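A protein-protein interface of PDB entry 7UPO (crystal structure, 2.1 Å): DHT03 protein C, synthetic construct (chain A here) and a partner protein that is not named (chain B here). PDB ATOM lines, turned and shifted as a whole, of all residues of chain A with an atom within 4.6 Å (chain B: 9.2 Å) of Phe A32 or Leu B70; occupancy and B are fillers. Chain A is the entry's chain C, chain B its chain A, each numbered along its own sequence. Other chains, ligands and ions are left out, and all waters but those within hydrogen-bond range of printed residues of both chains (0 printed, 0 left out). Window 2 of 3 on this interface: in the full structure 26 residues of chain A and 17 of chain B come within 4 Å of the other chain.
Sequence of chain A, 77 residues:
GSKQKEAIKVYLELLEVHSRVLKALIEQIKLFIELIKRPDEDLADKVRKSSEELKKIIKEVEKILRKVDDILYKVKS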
ATOM      1  N   GLN A  28      11.542   2.533  -6.178  1.00  0.00           N
ATOM      2  CA  GLN A  28      11.857   1.662  -7.308  1.00  0.00           C
ATOM      3  C   GLN A  28      10.821   1.790  -8.416  1.00  0.00           C
ATOM      4  O   GLN A  28      11.168   1.760  -9.601  1.00  0.00           O
ATOM      5  CB  GLN A  28      11.963   0.211  -6.848  1.00  0.00           C
ATOM      6  CG  GLN A  28      13.177  -0.083  -5.991  1.00  0.00           C
ATOM      7  CD  GLN A  28      13.454  -1.568  -5.877  1.00  0.00           C
ATOM      8  OE1 GLN A  28      13.062  -2.353  -6.741  1.00  0.00           O
ATOM      9  NE2 GLN A  28      14.132  -1.962  -4.804  1.00  0.00           N
ATOM     10  N   ILE A  29       9.544   1.927  -8.053  1.00  0.00           N
ATOM     11  CA  ILE A  29       8.503   2.058  -9.067  1.00  0.00           C
ATOM     12  C   ILE A  29       8.665   3.366  -9.832  1.00  0.00           C
ATOM     13  O   ILE A  29       8.565   3.396 -11.064  1.00  0.00           O
ATOM     14  CB  ILE A  29       7.108   1.945  -8.425  1.00  0.00           C
ATOM     15  CG1 ILE A  29       6.903   0.550  -7.833  1.00  0.00           C
ATOM     16  CG2 ILE A  29       6.029   2.240  -9.450  1.00  0.00           C
ATOM     17  CD1 ILE A  29       5.568   0.374  -7.144  1.00  0.00           C
ATOM     18  N   LYS A  30       8.925   4.464  -9.118  1.00  0.00           N
ATOM     19  CA  LYS A  30       9.164   5.740  -9.787  1.00  0.00           C
ATOM     20  C   LYS A  30      10.386   5.666 -10.692  1.00  0.00           C
ATOM     21  O   LYS A  30      10.388   6.228 -11.794  1.00  0.00           O
ATOM     22  CB  LYS A  30       9.341   6.853  -8.757  1.00  0.00           C
ATOM     23  CG  LYS A  30       8.103   7.186  -7.951  1.00  0.00           C
ATOM     24  CD  LYS A  30       8.424   8.269  -6.933  1.00  0.00           C
ATOM     25  CE  LYS A  30       7.193   8.687  -6.160  1.00  0.00           C
ATOM     26  NZ  LYS A  30       7.541   9.604  -5.042  1.00  0.00           N
ATOM     27  N   LEU A  31      11.440   4.983 -10.240  1.00  0.00           N
ATOM     28  CA  LEU A  31      12.651   4.876 -11.045  1.00  0.00           C
ATOM     29  C   LEU A  31      12.395   4.095 -12.327  1.00  0.00           C
ATOM     30  O   LEU A  31      12.909   4.453 -13.395  1.00  0.00           O
ATOM     31  CB  LEU A  31      13.766   4.224 -10.228  1.00  0.00           C
ATOM     32  CG  LEU A  31      14.339   5.086  -9.101  1.00  0.00           C
ATOM     33  CD1 LEU A  31      15.411   4.343  -8.318  1.00  0.00           C
ATOM     34  CD2 LEU A  31      14.884   6.381  -9.669  1.00  0.00           C
ATOM     35  N   PHE A  32      11.601   3.025 -12.246  1.00  0.00           N
ATOM     36  CA  PHE A  32      11.281   2.264 -13.447  1.00  0.00           C
ATOM     37  C   PHE A  32      10.368   3.045 -14.382  1.00  0.00           C
ATOM     38  O   PHE A  32      10.486   2.917 -15.604  1.00  0.00           O
ATOM     39  CB  PHE A  32      10.646   0.924 -13.077  1.00  0.00           C
ATOM     40  CG  PHE A  32      11.645  -0.147 -12.750  1.00  0.00           C
ATOM     41  CD1 PHE A  32      12.531  -0.596 -13.716  1.00  0.00           C
ATOM     42  CD2 PHE A  32      11.697  -0.710 -11.486  1.00  0.00           C
ATOM     43  CE1 PHE A  32      13.455  -1.583 -13.425  1.00  0.00           C
ATOM     44  CE2 PHE A  32      12.619  -1.697 -11.190  1.00  0.00           C
ATOM     45  CZ  PHE A  32      13.498  -2.135 -12.160  1.00  0.00           C
ATOM     46  N   ILE A  33       9.457   3.853 -13.831  1.00  0.00           N
ATOM     47  CA  ILE A  33       8.607   4.696 -14.670  1.00  0.00           C
ATOM     48  C   ILE A  33       9.463   5.597 -15.550  1.00  0.00           C
ATOM     49  O   ILE A  33       9.197   5.759 -16.747  1.00  0.00           O
ATOM     50  CB  ILE A  33       7.632   5.512 -13.801  1.00  0.00           C
ATOM     51  CG1 ILE A  33       6.586   4.597 -13.161  1.00  0.00           C
ATOM     52  CG2 ILE A  33       6.953   6.597 -14.628  1.00  0.00           C
ATOM     53  CD1 ILE A  33       5.718   5.292 -12.126  1.00  0.00           C
ATOM     54  N   GLU A  34      10.516   6.182 -14.977  1.00  0.00           N
ATOM     55  CA  GLU A  34      11.396   7.040 -15.759  1.00  0.00           C
ATOM     56  C   GLU A  34      12.342   6.233 -16.642  1.00  0.00           C
ATOM     57  O   GLU A  34      12.666   6.670 -17.752  1.00  0.00           O
ATOM     58  CB  GLU A  34      12.186   7.966 -14.833  1.00  0.00           C
ATOM     59  CG  GLU A  34      12.952   9.069 -15.555  1.00  0.00           C
ATOM     60  CD  GLU A  34      12.046  10.036 -16.289  1.00  0.00           C
ATOM     61  OE1 GLU A  34      10.980  10.387 -15.742  1.00  0.00           O
ATOM     62  OE2 GLU A  34      12.402  10.444 -17.416  1.00  0.00           O
ATOM     63  N   LEU A  35      12.786   5.060 -16.177  1.00  0.00           N
ATOM     64  CA  LEU A  35      13.651   4.216 -16.997  1.00  0.00           C
ATOM     65  C   LEU A  35      12.919   3.703 -18.232  1.00  0.00           C
ATOM     66  O   LEU A  35      13.510   3.601 -19.313  1.00  0.00           O
ATOM     67  CB  LEU A  35      14.180   3.044 -16.171  1.00  0.00           C
ATOM     68  CG  LEU A  35      15.417   3.298 -15.309  1.00  0.00           C
ATOM     69  CD1 LEU A  35      15.701   2.096 -14.423  1.00  0.00           C
ATOM     70  CD2 LEU A  35      16.614   3.609 -16.189  1.00  0.00           C
ATOM     71  N   ILE A  36      11.637   3.364 -18.086  1.00  0.00           N
ATOM     72  CA  ILE A  36      10.849   2.918 -19.230  1.00  0.00           C
ATOM     73  C   ILE A  36      10.628   4.069 -20.203  1.00  0.00           C
ATOM     74  O   ILE A  36      10.669   3.885 -21.426  1.00  0.00           O
ATOM     75  CB  ILE A  36       9.521   2.307 -18.749  1.00  0.00           C
ATOM     76  CG1 ILE A  36       9.785   1.008 -17.984  1.00  0.00           C
ATOM     77  CG2 ILE A  36       8.585   2.054 -19.920  1.00  0.00           C
ATOM     78  CD1 ILE A  36       8.693   0.640 -17.004  1.00  0.00           C
ATOM     79  N   VAL A  47      18.448   2.252  -8.755  1.00  0.00           N
ATOM     80  CA  VAL A  47      17.594   1.072  -8.644  1.00  0.00           C
ATOM     81  C   VAL A  47      18.354  -0.053  -7.957  1.00  0.00           C
ATOM     82  O   VAL A  47      17.839  -0.709  -7.042  1.00  0.00           O
ATOM     83  CB  VAL A  47      17.082   0.633 -10.029  1.00  0.00           C
ATOM     84  CG1 VAL A  47      16.317  -0.673  -9.915  1.00  0.00           C
ATOM     85  CG2 VAL A  47      16.200   1.697 -10.636  1.00  0.00           C
ATOM     86  N   GLU B   5      14.657 -14.411 -21.325  1.00  0.00           N
ATOM     87  CA  GLU B   5      14.551 -13.497 -20.192  1.00  0.00           C
ATOM     88  C   GLU B   5      13.109 -13.078 -19.937  1.00  0.00           C
ATOM     89  O   GLU B   5      12.717 -12.881 -18.782  1.00  0.00           O
ATOM     90  CB  GLU B   5      15.428 -12.261 -20.420  1.00  0.00           C
ATOM     91  CG  GLU B   5      16.908 -12.564 -20.608  1.00  0.00           C
ATOM     92  CD  GLU B   5      17.239 -13.024 -22.018  1.00  0.00           C
ATOM     93  OE1 GLU B   5      16.455 -12.719 -22.943  1.00  0.00           O
ATOM     94  OE2 GLU B   5      18.280 -13.691 -22.202  1.00  0.00           O
ATOM     95  N   GLU B   6      12.308 -12.934 -20.995  1.00  0.00           N
ATOM     96  CA  GLU B   6      10.902 -12.587 -20.815  1.00  0.00           C
ATOM     97  C   GLU B   6      10.127 -13.745 -20.199  1.00  0.00           C
ATOM     98  O   GLU B   6       9.220 -13.529 -19.387  1.00  0.00           O
ATOM     99  CB  GLU B   6      10.289 -12.180 -22.153  1.00  0.00           C
ATOM    100  CG  GLU B   6      10.966 -10.989 -22.803  1.00  0.00           C
ATOM    101  CD  GLU B   6      10.664 -10.891 -24.284  1.00  0.00           C
ATOM    102  OE1 GLU B   6       9.958 -11.780 -24.809  1.00  0.00           O
ATOM    103  OE2 GLU B   6      11.136  -9.930 -24.925  1.00  0.00           O
ATOM    104  N   LYS B   8      11.468 -15.962 -18.154  1.00  0.00           N
ATOM    105  CA  LYS B   8      11.884 -15.969 -16.754  1.00  0.00           C
ATOM    106  C   LYS B   8      11.113 -14.931 -15.947  1.00  0.00           C
ATOM    107  O   LYS B   8      10.760 -15.171 -14.787  1.00  0.00           O
ATOM    108  CB  LYS B   8      13.389 -15.721 -16.652  1.00  0.00           C
ATOM    109  CG  LYS B   8      13.921 -15.700 -15.228  1.00  0.00           C
ATOM    110  CD  LYS B   8      15.411 -15.394 -15.189  1.00  0.00           C
ATOM    111  CE  LYS B   8      16.221 -16.486 -15.867  1.00  0.00           C
ATOM    112  NZ  LYS B   8      17.685 -16.225 -15.780  1.00  0.00           N
ATOM    113  N   LEU B   9      10.835 -13.772 -16.551  1.00  0.00           N
ATOM    114  CA  LEU B   9      10.072 -12.744 -15.852  1.00  0.00           C
ATOM    115  C   LEU B   9       8.609 -13.146 -15.706  1.00  0.00           C
ATOM    116  O   LEU B   9       7.991 -12.884 -14.667  1.00  0.00           O
ATOM    117  CB  LEU B   9      10.201 -11.411 -16.590  1.00  0.00           C
ATOM    118  CG  LEU B   9       9.450 -10.204 -16.024  1.00  0.00           C
ATOM    119  CD1 LEU B   9      10.284  -8.946 -16.186  1.00  0.00           C
ATOM    120  CD2 LEU B   9       8.107 -10.039 -16.714  1.00  0.00           C
ATOM    121  N   LEU B  12       8.389 -15.674 -12.873  1.00  0.00           N
ATOM    122  CA  LEU B  12       8.454 -14.991 -11.585  1.00  0.00           C
ATOM    123  C   LEU B  12       7.206 -14.162 -11.328  1.00  0.00           C
ATOM    124  O   LEU B  12       6.787 -14.012 -10.174  1.00  0.00           O
ATOM    125  CB  LEU B  12       9.698 -14.106 -11.516  1.00  0.00           C
ATOM    126  CG  LEU B  12      10.937 -14.711 -10.853  1.00  0.00           C
ATOM    127  CD1 LEU B  12      11.534 -15.831 -11.697  1.00  0.00           C
ATOM    128  CD2 LEU B  12      11.964 -13.627 -10.585  1.00  0.00           C
ATOM    129  N   LEU B  13       6.597 -13.617 -12.383  1.00  0.00           N
ATOM    130  CA  LEU B  13       5.388 -12.824 -12.203  1.00  0.00           C
ATOM    131  C   LEU B  13       4.219 -13.698 -11.764  1.00  0.00           C
ATOM    132  O   LEU B  13       3.425 -13.295 -10.905  1.00  0.00           O
ATOM    133  CB  LEU B  13       5.054 -12.078 -13.494  1.00  0.00           C
ATOM    134  CG  LEU B  13       4.417 -10.698 -13.320  1.00  0.00           C
ATOM    135  CD1 LEU B  13       5.288  -9.815 -12.439  1.00  0.00           C
ATOM    136  CD2 LEU B  13       4.185 -10.042 -14.669  1.00  0.00           C
ATOM    137  N   LEU B  16       4.771 -14.480  -8.277  1.00  0.00           N
ATOM    138  CA  LEU B  16       4.445 -13.324  -7.450  1.00  0.00           C
ATOM    139  C   LEU B  16       2.944 -13.230  -7.208  1.00  0.00           C
ATOM    140  O   LEU B  16       2.508 -12.898  -6.099  1.00  0.00           O
ATOM    141  CB  LEU B  16       4.967 -12.048  -8.111  1.00  0.00           C
ATOM    142  CG  LEU B  16       4.948 -10.781  -7.259  1.00  0.00           C
ATOM    143  CD1 LEU B  16       5.801 -10.978  -6.023  1.00  0.00           C
ATOM    144  CD2 LEU B  16       5.434  -9.584  -8.062  1.00  0.00           C
ATOM    145  N   ILE B  62      11.184 -12.223  -4.186  1.00  0.00           N
ATOM    146  CA  ILE B  62      10.753 -12.192  -5.580  1.00  0.00           C
ATOM    147  C   ILE B  62      10.854 -10.777  -6.135  1.00  0.00           C
ATOM    148  O   ILE B  62      11.213 -10.577  -7.302  1.00  0.00           O
ATOM    149  CB  ILE B  62       9.328 -12.758  -5.715  1.00  0.00           C
ATOM    150  CG1 ILE B  62       9.285 -14.204  -5.221  1.00  0.00           C
ATOM    151  CG2 ILE B  62       8.857 -12.689  -7.159  1.00  0.00           C
ATOM    152  CD1 ILE B  62       7.905 -14.822  -5.262  1.00  0.00           C
ATOM    153  N   LEU B  63      10.546  -9.771  -5.309  1.00  0.00           N
ATOM    154  CA  LEU B  63      10.673  -8.386  -5.755  1.00  0.00           C
ATOM    155  C   LEU B  63      12.125  -8.036  -6.055  1.00  0.00           C
ATOM    156  O   LEU B  63      12.411  -7.335  -7.035  1.00  0.00           O
ATOM    157  CB  LEU B  63      10.102  -7.436  -4.703  1.00  0.00           C
ATOM    158  CG  LEU B  63       8.590  -7.461  -4.480  1.00  0.00           C
ATOM    159  CD1 LEU B  63       8.198  -6.440  -3.422  1.00  0.00           C
ATOM    160  CD2 LEU B  63       7.847  -7.200  -5.778  1.00  0.00           C
ATOM    161  N   VAL B  64      13.055  -8.508  -5.223  1.00  0.00           N
ATOM    162  CA  VAL B  64      14.471  -8.263  -5.476  1.00  0.00           C
ATOM    163  C   VAL B  64      14.890  -8.896  -6.796  1.00  0.00           C
ATOM    164  O   VAL B  64      15.594  -8.279  -7.606  1.00  0.00           O
ATOM    165  CB  VAL B  64      15.322  -8.783  -4.303  1.00  0.00           C
ATOM    166  CG1 VAL B  64      16.793  -8.784  -4.678  1.00  0.00           C
ATOM    167  CG2 VAL B  64      15.091  -7.933  -3.066  1.00  0.00           C
ATOM    168  N   GLU B  65      14.454 -10.133  -7.039  1.00  0.00           N
ATOM    169  CA  GLU B  65      14.807 -10.806  -8.284  1.00  0.00           C
ATOM    170  C   GLU B  65      14.073 -10.202  -9.475  1.00  0.00           C
ATOM    171  O   GLU B  65      14.620 -10.164 -10.582  1.00  0.00           O
ATOM    172  CB  GLU B  65      14.513 -12.302  -8.172  1.00  0.00           C
ATOM    173  CG  GLU B  65      15.228 -13.155  -9.207  1.00  0.00           C
ATOM    174  CD  GLU B  65      14.931 -14.633  -9.044  1.00  0.00           C
ATOM    175  OE1 GLU B  65      14.367 -15.015  -7.997  1.00  0.00           O
ATOM    176  OE2 GLU B  65      15.259 -15.413  -9.964  1.00  0.00           O
ATOM    177  N   LEU B  66      12.842  -9.725  -9.269  1.00  0.00           N
ATOM    178  CA  LEU B  66      12.114  -9.068 -10.350  1.00  0.00           C
ATOM    179  C   LEU B  66      12.783  -7.758 -10.746  1.00  0.00           C
ATOM    180  O   LEU B  66      12.812  -7.401 -11.930  1.00  0.00           O
ATOM    181  CB  LEU B  66      10.663  -8.821  -9.934  1.00  0.00           C
ATOM    182  CG  LEU B  66       9.717  -8.317 -11.027  1.00  0.00           C
ATOM    183  CD1 LEU B  66       9.350  -9.447 -11.982  1.00  0.00           C
ATOM    184  CD2 LEU B  66       8.472  -7.678 -10.424  1.00  0.00           C
ATOM    185  N   SER B  67      13.323  -7.027  -9.768  1.00  0.00           N
ATOM    186  CA  SER B  67      14.014  -5.779 -10.073  1.00  0.00           C
ATOM    187  C   SER B  67      15.272  -6.032 -10.894  1.00  0.00           C
ATOM    188  O   SER B  67      15.617  -5.236 -11.774  1.00  0.00           O
ATOM    189  CB  SER B  67      14.357  -5.039  -8.782  1.00  0.00           C
ATOM    190  OG  SER B  67      15.185  -3.921  -9.045  1.00  0.00           O
ATOM    191  N   ASP B  68      15.970  -7.135 -10.617  1.00  0.00           N
ATOM    192  CA  ASP B  68      17.173  -7.449 -11.379  1.00  0.00           C
ATOM    193  C   ASP B  68      16.836  -7.803 -12.822  1.00  0.00           C
ATOM    194  O   ASP B  68      17.517  -7.355 -13.751  1.00  0.00           O
ATOM    195  CB  ASP B  68      17.935  -8.593 -10.711  1.00  0.00           C
ATOM    196  CG  ASP B  68      19.193  -8.972 -11.467  1.00  0.00           C
ATOM    197  OD1 ASP B  68      20.160  -8.184 -11.448  1.00  0.00           O
ATOM    198  OD2 ASP B  68      19.212 -10.057 -12.088  1.00  0.00           O
ATOM    199  N   ILE B  69      15.785  -8.599 -13.029  1.00  0.00           N
ATOM    200  CA  ILE B  69      15.407  -8.994 -14.383  1.00  0.00           C
ATOM    201  C   ILE B  69      14.917  -7.788 -15.178  1.00  0.00           C
ATOM    202  O   ILE B  69      15.192  -7.666 -16.377  1.00  0.00           O
ATOM    203  CB  ILE B  69      14.350 -10.112 -14.333  1.00  0.00           C
ATOM    204  CG1 ILE B  69      14.909 -11.338 -13.606  1.00  0.00           C
ATOM    205  CG2 ILE B  69      13.895 -10.491 -15.735  1.00  0.00           C
ATOM    206  CD1 ILE B  69      13.925 -12.475 -13.487  1.00  0.00           C
ATOM    207  N   LEU B  70      14.195  -6.876 -14.524  1.00  0.00           N
ATOM    208  CA  LEU B  70      13.701  -5.692 -15.220  1.00  0.00           C
ATOM    209  C   LEU B  70      14.847  -4.801 -15.682  1.00  0.00           C
ATOM    210  O   LEU B  70      14.796  -4.234 -16.779  1.00  0.00           O
ATOM    211  CB  LEU B  70      12.742  -4.914 -14.321  1.00  0.00           C
ATOM    212  CG  LEU B  70      11.262  -5.285 -14.427  1.00  0.00           C
ATOM    213  CD1 LEU B  70      10.445  -4.531 -13.392  1.00  0.00           C
ATOM    214  CD2 LEU B  70      10.743  -5.002 -15.832  1.00  0.00           C
ATOM    215  N   LEU B  71      15.892  -4.667 -14.861  1.00  0.00           N
ATOM    216  CA  LEU B  71      17.042  -3.870 -15.274  1.00  0.00           C
ATOM    217  C   LEU B  71      17.775  -4.508 -16.446  1.00  0.00           C
ATOM    218  O   LEU B  71      18.308  -3.793 -17.302  1.00  0.00           O
ATOM    219  CB  LEU B  71      17.997  -3.662 -14.098  1.00  0.00           C
ATOM    220  CG  LEU B  71      17.714  -2.429 -13.239  1.00  0.00           C
ATOM    221  CD1 LEU B  71      18.755  -2.300 -12.144  1.00  0.00           C
ATOM    222  CD2 LEU B  71      17.675  -1.174 -14.099  1.00  0.00           C
ATOM    223  N   LYS B  72      17.815  -5.841 -16.505  1.00  0.00           N
ATOM    224  CA  LYS B  72      18.410  -6.505 -17.660  1.00  0.00           C
ATOM    225  C   LYS B  72      17.588  -6.259 -18.919  1.00  0.00           C
ATOM    226  O   LYS B  72      18.148  -5.999 -19.991  1.00  0.00           O
ATOM    227  CB  LYS B  72      18.551  -8.005 -17.393  1.00  0.00           C
ATOM    228  CG  LYS B  72      19.905  -8.435 -16.830  1.00  0.00           C
ATOM    229  CD  LYS B  72      20.120  -7.921 -15.414  1.00  0.00           C
ATOM    230  CE  LYS B  72      21.365  -8.517 -14.778  1.00  0.00           C
ATOM    231  NZ  LYS B  72      22.598  -8.139 -15.519  1.00  0.00           N
ATOM    232  N   LEU B  73      16.258  -6.329 -18.808  1.00  0.00           N
ATOM    233  CA  LEU B  73      15.401  -6.129 -19.974  1.00  0.00           C
ATOM    234  C   LEU B  73      15.479  -4.693 -20.478  1.00  0.00           C
ATOM    235  O   LEU B  73      15.750  -4.453 -21.660  1.00  0.00           O
ATOM    236  CB  LEU B  73      13.957  -6.508 -19.639  1.00  0.00           C
ATOM    237  CG  LEU B  73      13.590  -7.992 -19.725  1.00  0.00           C
ATOM    238  CD1 LEU B  73      12.137  -8.213 -19.336  1.00  0.00           C
ATOM    239  CD2 LEU B  73      13.857  -8.527 -21.123  1.00  0.00           C
ATOM    240  N   ILE B  74      15.246  -3.721 -19.592  1.00  0.00           N
ATOM    241  CA  ILE B  74      15.357  -2.314 -19.966  1.00  0.00           C
ATOM    242  C   ILE B  74      16.799  -1.898 -20.224  1.00  0.00           C
ATOM    243  O   ILE B  74      17.035  -0.793 -20.730  1.00  0.00           O
ATOM    244  CB  ILE B  74      14.706  -1.444 -18.868  1.00  0.00           C
ATOM    245  CG1 ILE B  74      13.353  -2.032 -18.466  1.00  0.00           C
ATOM    246  CG2 ILE B  74      14.495  -0.015 -19.349  1.00  0.00           C
ATOM    247  CD1 ILE B  74      12.660  -1.265 -17.358  1.00  0.00           C
ATOM    248  N   SER B  75      17.762  -2.762 -19.908  1.00  0.00           N
ATOM    249  CA  SER B  75      19.184  -2.488 -20.117  1.00  0.00           C
ATOM    250  C   SER B  75      19.633  -1.265 -19.324  1.00  0.00           C
ATOM    251  O   SER B  75      20.058  -0.259 -19.890  1.00  0.00           O
ATOM    252  CB  SER B  75      19.489  -2.299 -21.608  1.00  0.00           C
ATOM    253  OG  SER B  75      20.819  -1.850 -21.809  1.00  0.00           O
ATOM    254  OXT SER B  75      19.578  -1.260 -18.094  1.00  0.00           O
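Printed residues of chain A that touch a printed residue of chain B: Gln A28, Phe A32, Leu A35, Ile A36 and Val A47.
Hydrophobic or aromatic side chains of chain A that line the printed part of chain B: Phe A32, Leu A35, Ile A36 and Val A47.
Printed residues of chain B that touch a printed residue of chain A: Ser B67, Leu B70, Leu B71 and Ile B74.
Among the printed residues, no Asp or Glu carboxylate lies within 4 Å of a Lys or Arg side-chain nitrogen of the other chain.
Among the printed residues, pairs that only touch across the chains: Gln A28 with Ser B67, Phe A32 with Ser B67, Phe A32 with Leu B70, Phe A32 with Ile B74, Leu A35 with Leu B71, Leu A35 with Ile B74, Ile A36 with Ile B74, Val A47 with Ser B67 and Val A47 with Leu B71.
Of the printed residues of chain B, Gln A28 touches Ser B67.
Of chain B, only Ser B67, Leu B70 and Ile B74 come within 4 Å of Phe A32.
Of the printed residues of chain B, Leu A35 touches Leu B71 (3.8 Å) and Ile B74 (3.7 Å).
Of the printed residues of chain A, Ser B67 touches Gln A28, Phe A32 and Val A47.
Of chain A, only Phe A32 comes within 4 Å of Leu B70.
The nearest printed residue of chain A that does not touch Leu B70 is Ile A36 (6.1 Å).
The nearest printed residue of chain B that does not touch Val A47 is Asp B68 (6.5 Å).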
